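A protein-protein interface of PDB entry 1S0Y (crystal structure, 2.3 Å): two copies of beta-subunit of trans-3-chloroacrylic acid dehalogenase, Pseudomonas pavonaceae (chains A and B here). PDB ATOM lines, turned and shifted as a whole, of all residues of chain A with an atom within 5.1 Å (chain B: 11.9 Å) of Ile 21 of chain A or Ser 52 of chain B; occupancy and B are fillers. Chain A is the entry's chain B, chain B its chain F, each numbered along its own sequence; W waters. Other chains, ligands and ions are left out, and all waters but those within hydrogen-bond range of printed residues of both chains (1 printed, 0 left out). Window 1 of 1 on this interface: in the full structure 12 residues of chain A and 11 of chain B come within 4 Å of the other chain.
Water W1 lies within hydrogen-bond range of ND1 of His 46 of chain B (2.7 Å), O of Leu 43 of chain A (2.7 Å) and ND2 of Asn 50 of chain B (3.0 Å).
No position is printed for both chains.
CE of Lys 17 of chain A touches OD1 of Asn 50 of chain B (3.1 Å). Gln 18 of chain A touches Ile 57 of chain B. Ser 52 of chain B touches Ile 21 of chain A. NH2 of Arg 22 of chain A touches CG1 of Ile 57 of chain B, 3.7 Å away. CA of Gly 55 of chain B touches CD1 of Ile 25 of chain A (3.9 Å). O of Ser 52 of chain B touches CA of Asn 40 of chain A, 3.2 Å away. Asn 40 of chain A touches Ile 53 of chain B (OD1 to CA, 3.5 Å). Val 41 of chain A touches Asn 50 of chain B (O to O, 3.8 Å). O of Val 41 of chain A touches CA of Met 51 of chain B, at 3.7 Å.
OE1 of Gln 19 of chain A is in hydrogen-bond range of NH1 of Arg 22 of chain A (3.2 Å). The backbone carbonyl oxygen (O) of Arg 56 of chain B is in hydrogen-bond range of the side-chain hydroxyl (OG) of Ser 52 of chain B. O of Ile 53 of chain B sits at hydrogen-bond distance from NE of Arg 56 of chain B.
NE2 of Gln 18 of chain A sits at hydrogen-bond distance from O of Ala 49 of chain B (2.9 Å). O of His 58 of chain B lies close to OE1 of Gln 18 of chain A, 3.4 Å away. The backbone carbonyl oxygen (O) of Ile 39 of chain A sits at hydrogen-bond distance from the backbone NH (N) of Ser 54 of chain B, 3.2 Å away. O of Ile 39 of chain A is in hydrogen-bond range of N of Gly 55 of chain B (2.9 Å). The side-chain amide oxygen (OD1) of Asn 40 of chain A is in hydrogen-bond range of the backbone NH (N) of Ser 54 of chain B (3.1 Å). The backbone carbonyl oxygen (O) of Ser 52 of chain B is in hydrogen-bond range of the backbone NH (N) of Val 41 of chain A (2.9 Å). O of Asn 50 of chain B lies within hydrogen-bond range of N of Leu 43 of chain A (2.9 Å).
Arg 16 of chain A touches none of the printed residues of chain B. Printed residues of chain B within 4 Å of Lys 17 of chain A: Asn 50. Of chain B, only Ala 49, Ile 57 and His 58 come within 4 Å of Gln 18 of chain A. No residue of chain B comes within 4 Å of Gln 19 of chain A. No residue of chain B comes within 4 Å of Leu 20 of chain A. Of chain B, only Ser 52 comes within 4 Å of Ile 21 of chain A. Of chain B, only Ile 57 (3.7 Å) comes within 4 Å of Arg 22 of chain A. No residue of chain B comes within 4 Å of Asp 23 of chain A. Ile 25 of chain A touches one residue of chain B. Asp 26 of chain A touches none of the printed residues of chain B. Of chain B, only Ser 52 (3.2 Å), Ile 53 (3.5 Å) and Ser 54 (3.1 Å) come within 4 Å of Asn 40 of chain A. Of the printed residues of chain B, Val 41 of chain A touches Asn 50 (3.8 Å), Met 51 (3.7 Å) and Ser 52 (2.9 Å). Of chain A, only Ile 21 (3.6 Å), Asn 40 (3.2 Å) and Val 41 (2.9 Å) come within 4 Å of Ser 52 of chain B. Printed residues of chain A within 4 Å of His 58 of chain B: Gln 18 (3.4 Å). The nearest residue of chain B that does not touch Ile 21 of chain A is Ala 49 of chain B (4.4 Å).
Hydrophobic or aromatic side chains of chain A within 4 Å of the printed part of chain B: Ile 21, Ile 25 and Leu 43. Among the printed residues, 16 pairs touch across the chains. Among the printed residues, no Asp or Glu carboxylate lies within 4 Å of a Lys or Arg side-chain nitrogen of the other chain.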
ATOM      1  N   ARG A  16       3.333 -19.223 -23.281  1.00  0.00           N
ATOM      2  CA  ARG A  16       4.109 -18.586 -24.342  1.00  0.00           C
ATOM      3  C   ARG A  16       5.013 -19.570 -25.075  1.00  0.00           C
ATOM      4  O   ARG A  16       5.214 -19.448 -26.281  1.00  0.00           O
ATOM      5  CB  ARG A  16       4.967 -17.460 -23.776  1.00  0.00           C
ATOM      6  CG  ARG A  16       4.521 -16.090 -24.210  1.00  0.00           C
ATOM      7  CD  ARG A  16       4.551 -15.950 -25.722  1.00  0.00           C
ATOM      8  NE  ARG A  16       5.224 -14.716 -26.123  1.00  0.00           N
ATOM      9  CZ  ARG A  16       4.868 -13.496 -25.722  1.00  0.00           C
ATOM     10  NH1 ARG A  16       3.835 -13.329 -24.901  1.00  0.00           N
ATOM     11  NH2 ARG A  16       5.554 -12.438 -26.142  1.00  0.00           N
ATOM     12  N   LYS A  17       5.562 -20.533 -24.342  1.00  0.00           N
ATOM     13  CA  LYS A  17       6.433 -21.530 -24.951  1.00  0.00           C
ATOM     14  C   LYS A  17       5.626 -22.422 -25.896  1.00  0.00           C
ATOM     15  O   LYS A  17       6.119 -22.849 -26.934  1.00  0.00           O
ATOM     16  CB  LYS A  17       7.129 -22.351 -23.862  1.00  0.00           C
ATOM     17  CG  LYS A  17       8.230 -21.571 -23.143  1.00  0.00           C
ATOM     18  CD  LYS A  17       8.294 -21.882 -21.646  1.00  0.00           C
ATOM     19  CE  LYS A  17       8.691 -23.320 -21.352  1.00  0.00           C
ATOM     20  NZ  LYS A  17       8.789 -23.539 -19.883  1.00  0.00           N
ATOM     21  N   GLN A  18       4.372 -22.669 -25.548  1.00  0.00           N
ATOM     22  CA  GLN A  18       3.495 -23.488 -26.386  1.00  0.00           C
ATOM     23  C   GLN A  18       3.191 -22.749 -27.689  1.00  0.00           C
ATOM     24  O   GLN A  18       3.048 -23.352 -28.750  1.00  0.00           O
ATOM     25  CB  GLN A  18       2.189 -23.779 -25.646  1.00  0.00           C
ATOM     26  CG  GLN A  18       2.358 -24.672 -24.433  1.00  0.00           C
ATOM     27  CD  GLN A  18       2.537 -26.127 -24.817  1.00  0.00           C
ATOM     28  OE1 GLN A  18       1.616 -26.760 -25.347  1.00  0.00           O
ATOM     29  NE2 GLN A  18       3.726 -26.665 -24.561  1.00  0.00           N
ATOM     30  N   GLN A  19       3.089 -21.432 -27.592  1.00  0.00           N
ATOM     31  CA  GLN A  19       2.812 -20.604 -28.751  1.00  0.00           C
ATOM     32  C   GLN A  19       4.053 -20.561 -29.635  1.00  0.00           C
ATOM     33  O   GLN A  19       3.943 -20.635 -30.857  1.00  0.00           O
ATOM     34  CB  GLN A  19       2.424 -19.188 -28.311  1.00  0.00           C
ATOM     35  CG  GLN A  19       2.043 -18.271 -29.473  1.00  0.00           C
ATOM     36  CD  GLN A  19       0.879 -18.819 -30.268  1.00  0.00           C
ATOM     37  OE1 GLN A  19      -0.180 -19.088 -29.716  1.00  0.00           O
ATOM     38  NE2 GLN A  19       1.070 -18.988 -31.570  1.00  0.00           N
ATOM     39  N   LEU A  20       5.230 -20.436 -29.015  1.00  0.00           N
ATOM     40  CA  LEU A  20       6.486 -20.409 -29.764  1.00  0.00           C
ATOM     41  C   LEU A  20       6.690 -21.740 -30.500  1.00  0.00           C
ATOM     42  O   LEU A  20       7.244 -21.765 -31.597  1.00  0.00           O
ATOM     43  CB  LEU A  20       7.675 -20.139 -28.827  1.00  0.00           C
ATOM     44  CG  LEU A  20       9.089 -20.364 -29.396  1.00  0.00           C
ATOM     45  CD1 LEU A  20       9.322 -19.490 -30.643  1.00  0.00           C
ATOM     46  CD2 LEU A  20      10.128 -20.049 -28.328  1.00  0.00           C
ATOM     47  N   ILE A  21       6.242 -22.845 -29.903  1.00  0.00           N
ATOM     48  CA  ILE A  21       6.388 -24.141 -30.567  1.00  0.00           C
ATOM     49  C   ILE A  21       5.514 -24.111 -31.816  1.00  0.00           C
ATOM     50  O   ILE A  21       5.971 -24.412 -32.917  1.00  0.00           O
ATOM     51  CB  ILE A  21       5.911 -25.332 -29.695  1.00  0.00           C
ATOM     52  CG1 ILE A  21       6.791 -25.482 -28.451  1.00  0.00           C
ATOM     53  CG2 ILE A  21       5.909 -26.609 -30.532  1.00  0.00           C
ATOM     54  CD1 ILE A  21       8.257 -25.554 -28.732  1.00  0.00           C
ATOM     55  N   ARG A  22       4.250 -23.743 -31.632  1.00  0.00           N
ATOM     56  CA  ARG A  22       3.325 -23.676 -32.747  1.00  0.00           C
ATOM     57  C   ARG A  22       3.883 -22.760 -33.845  1.00  0.00           C
ATOM     58  O   ARG A  22       3.846 -23.105 -35.029  1.00  0.00           O
ATOM     59  CB  ARG A  22       1.960 -23.179 -32.255  1.00  0.00           C
ATOM     60  CG  ARG A  22       0.909 -23.061 -33.352  1.00  0.00           C
ATOM     61  CD  ARG A  22      -0.522 -22.952 -32.801  1.00  0.00           C
ATOM     62  NE  ARG A  22      -0.591 -22.270 -31.511  1.00  0.00           N
ATOM     63  CZ  ARG A  22      -0.620 -22.899 -30.341  1.00  0.00           C
ATOM     64  NH1 ARG A  22      -0.678 -22.207 -29.211  1.00  0.00           N
ATOM     65  NH2 ARG A  22      -0.604 -24.224 -30.304  1.00  0.00           N
ATOM     66  N   ASP A  23       4.422 -21.609 -33.441  1.00  0.00           N
ATOM     67  CA  ASP A  23       4.984 -20.650 -34.385  1.00  0.00           C
ATOM     68  C   ASP A  23       6.131 -21.258 -35.194  1.00  0.00           C
ATOM     69  O   ASP A  23       6.278 -20.977 -36.385  1.00  0.00           O
ATOM     70  CB  ASP A  23       5.465 -19.388 -33.648  1.00  0.00           C
ATOM     71  CG  ASP A  23       4.311 -18.582 -33.037  1.00  0.00           C
ATOM     72  OD1 ASP A  23       3.177 -18.663 -33.571  1.00  0.00           O
ATOM     73  OD2 ASP A  23       4.541 -17.853 -32.035  1.00  0.00           O
ATOM     74  N   VAL A  24       6.939 -22.096 -34.548  1.00  0.00           N
ATOM     75  CA  VAL A  24       8.055 -22.734 -35.232  1.00  0.00           C
ATOM     76  C   VAL A  24       7.541 -23.758 -36.243  1.00  0.00           C
ATOM     77  O   VAL A  24       8.038 -23.828 -37.365  1.00  0.00           O
ATOM     78  CB  VAL A  24       9.014 -23.419 -34.234  1.00  0.00           C
ATOM     79  CG1 VAL A  24      10.050 -24.258 -34.982  1.00  0.00           C
ATOM     80  CG2 VAL A  24       9.715 -22.367 -33.392  1.00  0.00           C
ATOM     81  N   ILE A  25       6.548 -24.549 -35.850  1.00  0.00           N
ATOM     82  CA  ILE A  25       5.986 -25.544 -36.759  1.00  0.00           C
ATOM     83  C   ILE A  25       5.537 -24.791 -38.007  1.00  0.00           C
ATOM     84  O   ILE A  25       6.006 -25.037 -39.117  1.00  0.00           O
ATOM     85  CB  ILE A  25       4.731 -26.228 -36.163  1.00  0.00           C
ATOM     86  CG1 ILE A  25       5.070 -26.931 -34.845  1.00  0.00           C
ATOM     87  CG2 ILE A  25       4.143 -27.191 -37.181  1.00  0.00           C
ATOM     88  CD1 ILE A  25       6.161 -27.945 -34.956  1.00  0.00           C
ATOM     89  N   ASP A  26       4.624 -23.855 -37.776  1.00  0.00           N
ATOM     90  CA  ASP A  26       4.026 -23.010 -38.794  1.00  0.00           C
ATOM     91  C   ASP A  26       4.969 -22.391 -39.831  1.00  0.00           C
ATOM     92  O   ASP A  26       4.771 -22.583 -41.033  1.00  0.00           O
ATOM     93  CB  ASP A  26       3.223 -21.894 -38.109  1.00  0.00           C
ATOM     94  CG  ASP A  26       2.721 -20.844 -39.088  1.00  0.00           C
ATOM     95  OD1 ASP A  26       1.891 -21.189 -39.965  1.00  0.00           O
ATOM     96  OD2 ASP A  26       3.164 -19.677 -38.978  1.00  0.00           O
ATOM     97  N   ILE A  39       7.677 -32.447 -38.687  1.00  0.00           N
ATOM     98  CA  ILE A  39       8.374 -31.365 -37.991  1.00  0.00           C
ATOM     99  C   ILE A  39       8.512 -31.745 -36.514  1.00  0.00           C
ATOM    100  O   ILE A  39       7.556 -32.201 -35.888  1.00  0.00           O
ATOM    101  CB  ILE A  39       7.575 -30.024 -38.035  1.00  0.00           C
ATOM    102  CG1 ILE A  39       7.042 -29.749 -39.443  1.00  0.00           C
ATOM    103  CG2 ILE A  39       8.463 -28.868 -37.556  1.00  0.00           C
ATOM    104  CD1 ILE A  39       8.079 -29.362 -40.446  1.00  0.00           C
ATOM    105  N   ASN A  40       9.697 -31.546 -35.955  1.00  0.00           N
ATOM    106  CA  ASN A  40       9.925 -31.845 -34.546  1.00  0.00           C
ATOM    107  C   ASN A  40      10.567 -30.620 -33.914  1.00  0.00           C
ATOM    108  O   ASN A  40      11.477 -30.021 -34.497  1.00  0.00           O
ATOM    109  CB  ASN A  40      10.847 -33.054 -34.409  1.00  0.00           C
ATOM    110  CG  ASN A  40      10.302 -34.279 -35.113  1.00  0.00           C
ATOM    111  OD1 ASN A  40       9.262 -34.816 -34.741  1.00  0.00           O
ATOM    112  ND2 ASN A  40      11.000 -34.722 -36.144  1.00  0.00           N
ATOM    113  N   VAL A  41      10.101 -30.241 -32.728  1.00  0.00           N
ATOM    114  CA  VAL A  41      10.647 -29.066 -32.042  1.00  0.00           C
ATOM    115  C   VAL A  41      11.064 -29.380 -30.606  1.00  0.00           C
ATOM    116  O   VAL A  41      10.353 -30.069 -29.878  1.00  0.00           O
ATOM    117  CB  VAL A  41       9.620 -27.892 -32.006  1.00  0.00           C
ATOM    118  CG1 VAL A  41      10.228 -26.689 -31.306  1.00  0.00           C
ATOM    119  CG2 VAL A  41       9.193 -27.512 -33.422  1.00  0.00           C
ATOM    120  N   LEU A  43      12.357 -27.307 -27.264  1.00  0.00           N
ATOM    121  CA  LEU A  43      12.578 -26.025 -26.624  1.00  0.00           C
ATOM    122  C   LEU A  43      13.444 -26.271 -25.382  1.00  0.00           C
ATOM    123  O   LEU A  43      13.092 -27.078 -24.525  1.00  0.00           O
ATOM    124  CB  LEU A  43      11.233 -25.420 -26.223  1.00  0.00           C
ATOM    125  CG  LEU A  43      11.049 -23.920 -26.439  1.00  0.00           C
ATOM    126  CD1 LEU A  43       9.717 -23.478 -25.848  1.00  0.00           C
ATOM    127  CD2 LEU A  43      12.198 -23.165 -25.779  1.00  0.00           C
ATOM    128  N   HIS B   7      16.981 -37.164 -25.853  1.00  0.00           N
ATOM    129  CA  HIS B   7      16.122 -36.166 -25.227  1.00  0.00           C
ATOM    130  C   HIS B   7      14.807 -36.837 -24.874  1.00  0.00           C
ATOM    131  O   HIS B   7      13.985 -37.085 -25.757  1.00  0.00           O
ATOM    132  CB  HIS B   7      15.873 -35.008 -26.196  1.00  0.00           C
ATOM    133  CG  HIS B   7      17.103 -34.218 -26.515  1.00  0.00           C
ATOM    134  ND1 HIS B   7      17.666 -33.327 -25.628  1.00  0.00           N
ATOM    135  CD2 HIS B   7      17.909 -34.225 -27.605  1.00  0.00           C
ATOM    136  CE1 HIS B   7      18.766 -32.821 -26.157  1.00  0.00           C
ATOM    137  NE2 HIS B   7      18.935 -33.350 -27.355  1.00  0.00           N
ATOM    138  N   ILE B   8      14.612 -37.121 -23.586  1.00  0.00           N
ATOM    139  CA  ILE B   8      13.405 -37.805 -23.115  1.00  0.00           C
ATOM    140  C   ILE B   8      12.613 -36.998 -22.098  1.00  0.00           C
ATOM    141  O   ILE B   8      13.085 -35.986 -21.584  1.00  0.00           O
ATOM    142  CB  ILE B   8      13.746 -39.183 -22.478  1.00  0.00           C
ATOM    143  CG1 ILE B   8      14.391 -38.997 -21.099  1.00  0.00           C
ATOM    144  CG2 ILE B   8      14.714 -39.937 -23.365  1.00  0.00           C
ATOM    145  CD1 ILE B   8      14.601 -40.302 -20.337  1.00  0.00           C
ATOM    146  N   ALA B   9      11.397 -37.449 -21.811  1.00  0.00           N
ATOM    147  CA  ALA B   9      10.554 -36.759 -20.845  1.00  0.00           C
ATOM    148  C   ALA B   9      10.977 -37.117 -19.434  1.00  0.00           C
ATOM    149  O   ALA B   9      11.443 -38.222 -19.176  1.00  0.00           O
ATOM    150  CB  ALA B   9       9.085 -37.133 -21.054  1.00  0.00           C
ATOM    151  N   GLU B  45      16.692 -34.882 -19.877  1.00  0.00           N
ATOM    152  CA  GLU B  45      15.248 -34.905 -19.704  1.00  0.00           C
ATOM    153  C   GLU B  45      14.670 -33.506 -19.895  1.00  0.00           C
ATOM    154  O   GLU B  45      15.360 -32.511 -19.698  1.00  0.00           O
ATOM    155  CB  GLU B  45      14.909 -35.423 -18.304  1.00  0.00           C
ATOM    156  CG  GLU B  45      15.797 -36.573 -17.830  1.00  0.00           C
ATOM    157  CD  GLU B  45      15.650 -36.846 -16.343  1.00  0.00           C
ATOM    158  OE1 GLU B  45      14.661 -37.495 -15.935  1.00  0.00           O
ATOM    159  OE2 GLU B  45      16.526 -36.390 -15.572  1.00  0.00           O
ATOM    160  N   HIS B  46      13.403 -33.443 -20.289  1.00  0.00           N
ATOM    161  CA  HIS B  46      12.718 -32.174 -20.507  1.00  0.00           C
ATOM    162  C   HIS B  46      11.279 -32.309 -20.057  1.00  0.00           C
ATOM    163  O   HIS B  46      10.760 -33.420 -19.913  1.00  0.00           O
ATOM    164  CB  HIS B  46      12.674 -31.821 -21.993  1.00  0.00           C
ATOM    165  CG  HIS B  46      13.998 -31.880 -22.675  1.00  0.00           C
ATOM    166  ND1 HIS B  46      14.861 -30.807 -22.722  1.00  0.00           N
ATOM    167  CD2 HIS B  46      14.602 -32.884 -23.354  1.00  0.00           C
ATOM    168  CE1 HIS B  46      15.938 -31.146 -23.406  1.00  0.00           C
ATOM    169  NE2 HIS B  46      15.806 -32.400 -23.801  1.00  0.00           N
ATOM    170  N   ALA B  47      10.629 -31.169 -19.866  1.00  0.00           N
ATOM    171  CA  ALA B  47       9.227 -31.155 -19.501  1.00  0.00           C
ATOM    172  C   ALA B  47       8.499 -31.478 -20.808  1.00  0.00           C
ATOM    173  O   ALA B  47       8.887 -31.001 -21.886  1.00  0.00           O
ATOM    174  CB  ALA B  47       8.828 -29.780 -18.998  1.00  0.00           C
ATOM    175  N   GLU B  48       7.458 -32.299 -20.714  1.00  0.00           N
ATOM    176  CA  GLU B  48       6.692 -32.692 -21.888  1.00  0.00           C
ATOM    177  C   GLU B  48       6.360 -31.493 -22.769  1.00  0.00           C
ATOM    178  O   GLU B  48       6.530 -31.549 -23.975  1.00  0.00           O
ATOM    179  CB  GLU B  48       5.403 -33.382 -21.457  1.00  0.00           C
ATOM    180  CG  GLU B  48       5.615 -34.680 -20.702  1.00  0.00           C
ATOM    181  CD  GLU B  48       5.832 -35.868 -21.618  1.00  0.00           C
ATOM    182  OE1 GLU B  48       5.831 -37.015 -21.107  1.00  0.00           O
ATOM    183  OE2 GLU B  48       6.000 -35.657 -22.843  1.00  0.00           O
ATOM    184  N   ALA B  49       5.906 -30.406 -22.153  1.00  0.00           N
ATOM    185  CA  ALA B  49       5.529 -29.196 -22.877  1.00  0.00           C
ATOM    186  C   ALA B  49       6.608 -28.595 -23.786  1.00  0.00           C
ATOM    187  O   ALA B  49       6.284 -27.934 -24.773  1.00  0.00           O
ATOM    188  CB  ALA B  49       5.044 -28.147 -21.897  1.00  0.00           C
ATOM    189  N   ASN B  50       7.879 -28.801 -23.454  1.00  0.00           N
ATOM    190  CA  ASN B  50       8.955 -28.278 -24.282  1.00  0.00           C
ATOM    191  C   ASN B  50       9.229 -29.196 -25.467  1.00  0.00           C
ATOM    192  O   ASN B  50      10.164 -28.954 -26.225  1.00  0.00           O
ATOM    193  CB  ASN B  50      10.259 -28.151 -23.496  1.00  0.00           C
ATOM    194  CG  ASN B  50      10.169 -27.167 -22.353  1.00  0.00           C
ATOM    195  OD1 ASN B  50       9.471 -26.165 -22.435  1.00  0.00           O
ATOM    196  ND2 ASN B  50      10.904 -27.440 -21.284  1.00  0.00           N
ATOM    197  N   MET B  51       8.439 -30.251 -25.634  1.00  0.00           N
ATOM    198  CA  MET B  51       8.687 -31.171 -26.744  1.00  0.00           C
ATOM    199  C   MET B  51       7.531 -31.373 -27.727  1.00  0.00           C
ATOM    200  O   MET B  51       6.384 -31.598 -27.334  1.00  0.00           O
ATOM    201  CB  MET B  51       9.124 -32.537 -26.200  1.00  0.00           C
ATOM    202  CG  MET B  51      10.249 -32.484 -25.184  1.00  0.00           C
ATOM    203  SD  MET B  51      10.729 -34.148 -24.630  1.00  0.00           S
ATOM    204  CE  MET B  51       9.280 -34.590 -23.677  1.00  0.00           C
ATOM    205  N   SER B  52       7.846 -31.301 -29.015  1.00  0.00           N
ATOM    206  CA  SER B  52       6.841 -31.502 -30.056  1.00  0.00           C
ATOM    207  C   SER B  52       7.315 -32.506 -31.100  1.00  0.00           C
ATOM    208  O   SER B  52       8.329 -32.295 -31.765  1.00  0.00           O
ATOM    209  CB  SER B  52       6.503 -30.184 -30.752  1.00  0.00           C
ATOM    210  OG  SER B  52       5.551 -30.398 -31.783  1.00  0.00           O
ATOM    211  N   ILE B  53       6.582 -33.608 -31.222  1.00  0.00           N
ATOM    212  CA  ILE B  53       6.902 -34.638 -32.197  1.00  0.00           C
ATOM    213  C   ILE B  53       5.799 -34.668 -33.244  1.00  0.00           C
ATOM    214  O   ILE B  53       4.613 -34.652 -32.905  1.00  0.00           O
ATOM    215  CB  ILE B  53       6.993 -36.042 -31.571  1.00  0.00           C
ATOM    216  CG1 ILE B  53       8.193 -36.126 -30.622  1.00  0.00           C
ATOM    217  CG2 ILE B  53       7.110 -37.086 -32.690  1.00  0.00           C
ATOM    218  CD1 ILE B  53       9.530 -35.911 -31.299  1.00  0.00           C
ATOM    219  N   SER B  54       6.201 -34.712 -34.514  1.00  0.00           N
ATOM    220  CA  SER B  54       5.264 -34.743 -35.631  1.00  0.00           C
ATOM    221  C   SER B  54       4.280 -33.582 -35.564  1.00  0.00           C
ATOM    222  O   SER B  54       3.094 -33.758 -35.841  1.00  0.00           O
ATOM    223  CB  SER B  54       4.496 -36.069 -35.644  1.00  0.00           C
ATOM    224  OG  SER B  54       5.385 -37.175 -35.695  1.00  0.00           O
ATOM    225  N   GLY B  55       4.779 -32.409 -35.173  1.00  0.00           N
ATOM    226  CA  GLY B  55       3.953 -31.214 -35.096  1.00  0.00           C
ATOM    227  C   GLY B  55       2.849 -31.173 -34.053  1.00  0.00           C
ATOM    228  O   GLY B  55       2.036 -30.248 -34.048  1.00  0.00           O
ATOM    229  N   ARG B  56       2.816 -32.162 -33.169  1.00  0.00           N
ATOM    230  CA  ARG B  56       1.796 -32.217 -32.130  1.00  0.00           C
ATOM    231  C   ARG B  56       2.063 -31.219 -31.004  1.00  0.00           C
ATOM    232  O   ARG B  56       3.198 -31.039 -30.587  1.00  0.00           O
ATOM    233  CB  ARG B  56       1.706 -33.637 -31.557  1.00  0.00           C
ATOM    234  CG  ARG B  56       0.607 -34.504 -32.172  1.00  0.00           C
ATOM    235  CD  ARG B  56       1.147 -35.760 -32.839  1.00  0.00           C
ATOM    236  NE  ARG B  56       2.088 -36.474 -31.986  1.00  0.00           N
ATOM    237  CZ  ARG B  56       2.711 -37.598 -32.331  1.00  0.00           C
ATOM    238  NH1 ARG B  56       2.492 -38.151 -33.516  1.00  0.00           N
ATOM    239  NH2 ARG B  56       3.570 -38.164 -31.494  1.00  0.00           N
ATOM    240  N   ILE B  57       1.010 -30.565 -30.527  1.00  0.00           N
ATOM    241  CA  ILE B  57       1.120 -29.593 -29.444  1.00  0.00           C
ATOM    242  C   ILE B  57       0.572 -30.219 -28.171  1.00  0.00           C
ATOM    243  O   ILE B  57      -0.555 -30.712 -28.147  1.00  0.00           O
ATOM    244  CB  ILE B  57       0.332 -28.289 -29.766  1.00  0.00           C
ATOM    245  CG1 ILE B  57       1.131 -27.420 -30.742  1.00  0.00           C
ATOM    246  CG2 ILE B  57       0.048 -27.504 -28.496  1.00  0.00           C
ATOM    247  CD1 ILE B  57       1.277 -28.006 -32.127  1.00  0.00           C
ATOM    248  N   HIS B  58       1.372 -30.195 -27.110  1.00  0.00           N
ATOM    249  CA  HIS B  58       0.964 -30.790 -25.843  1.00  0.00           C
ATOM    250  C   HIS B  58      -0.370 -30.242 -25.334  1.00  0.00           C
ATOM    251  O   HIS B  58      -0.796 -29.161 -25.809  1.00  0.00           O
ATOM    252  CB  HIS B  58       2.060 -30.574 -24.795  1.00  0.00           C
ATOM    253  CG  HIS B  58       1.862 -31.370 -23.545  1.00  0.00           C
ATOM    254  ND1 HIS B  58       1.377 -30.818 -22.379  1.00  0.00           N
ATOM    255  CD2 HIS B  58       2.045 -32.688 -23.293  1.00  0.00           C
ATOM    256  CE1 HIS B  58       1.269 -31.763 -21.461  1.00  0.00           C
ATOM    257  NE2 HIS B  58       1.666 -32.907 -21.991  1.00  0.00           N
HETATM  258  O   HOH W   1      13.493 -28.540 -22.286  1.00  0.00           O
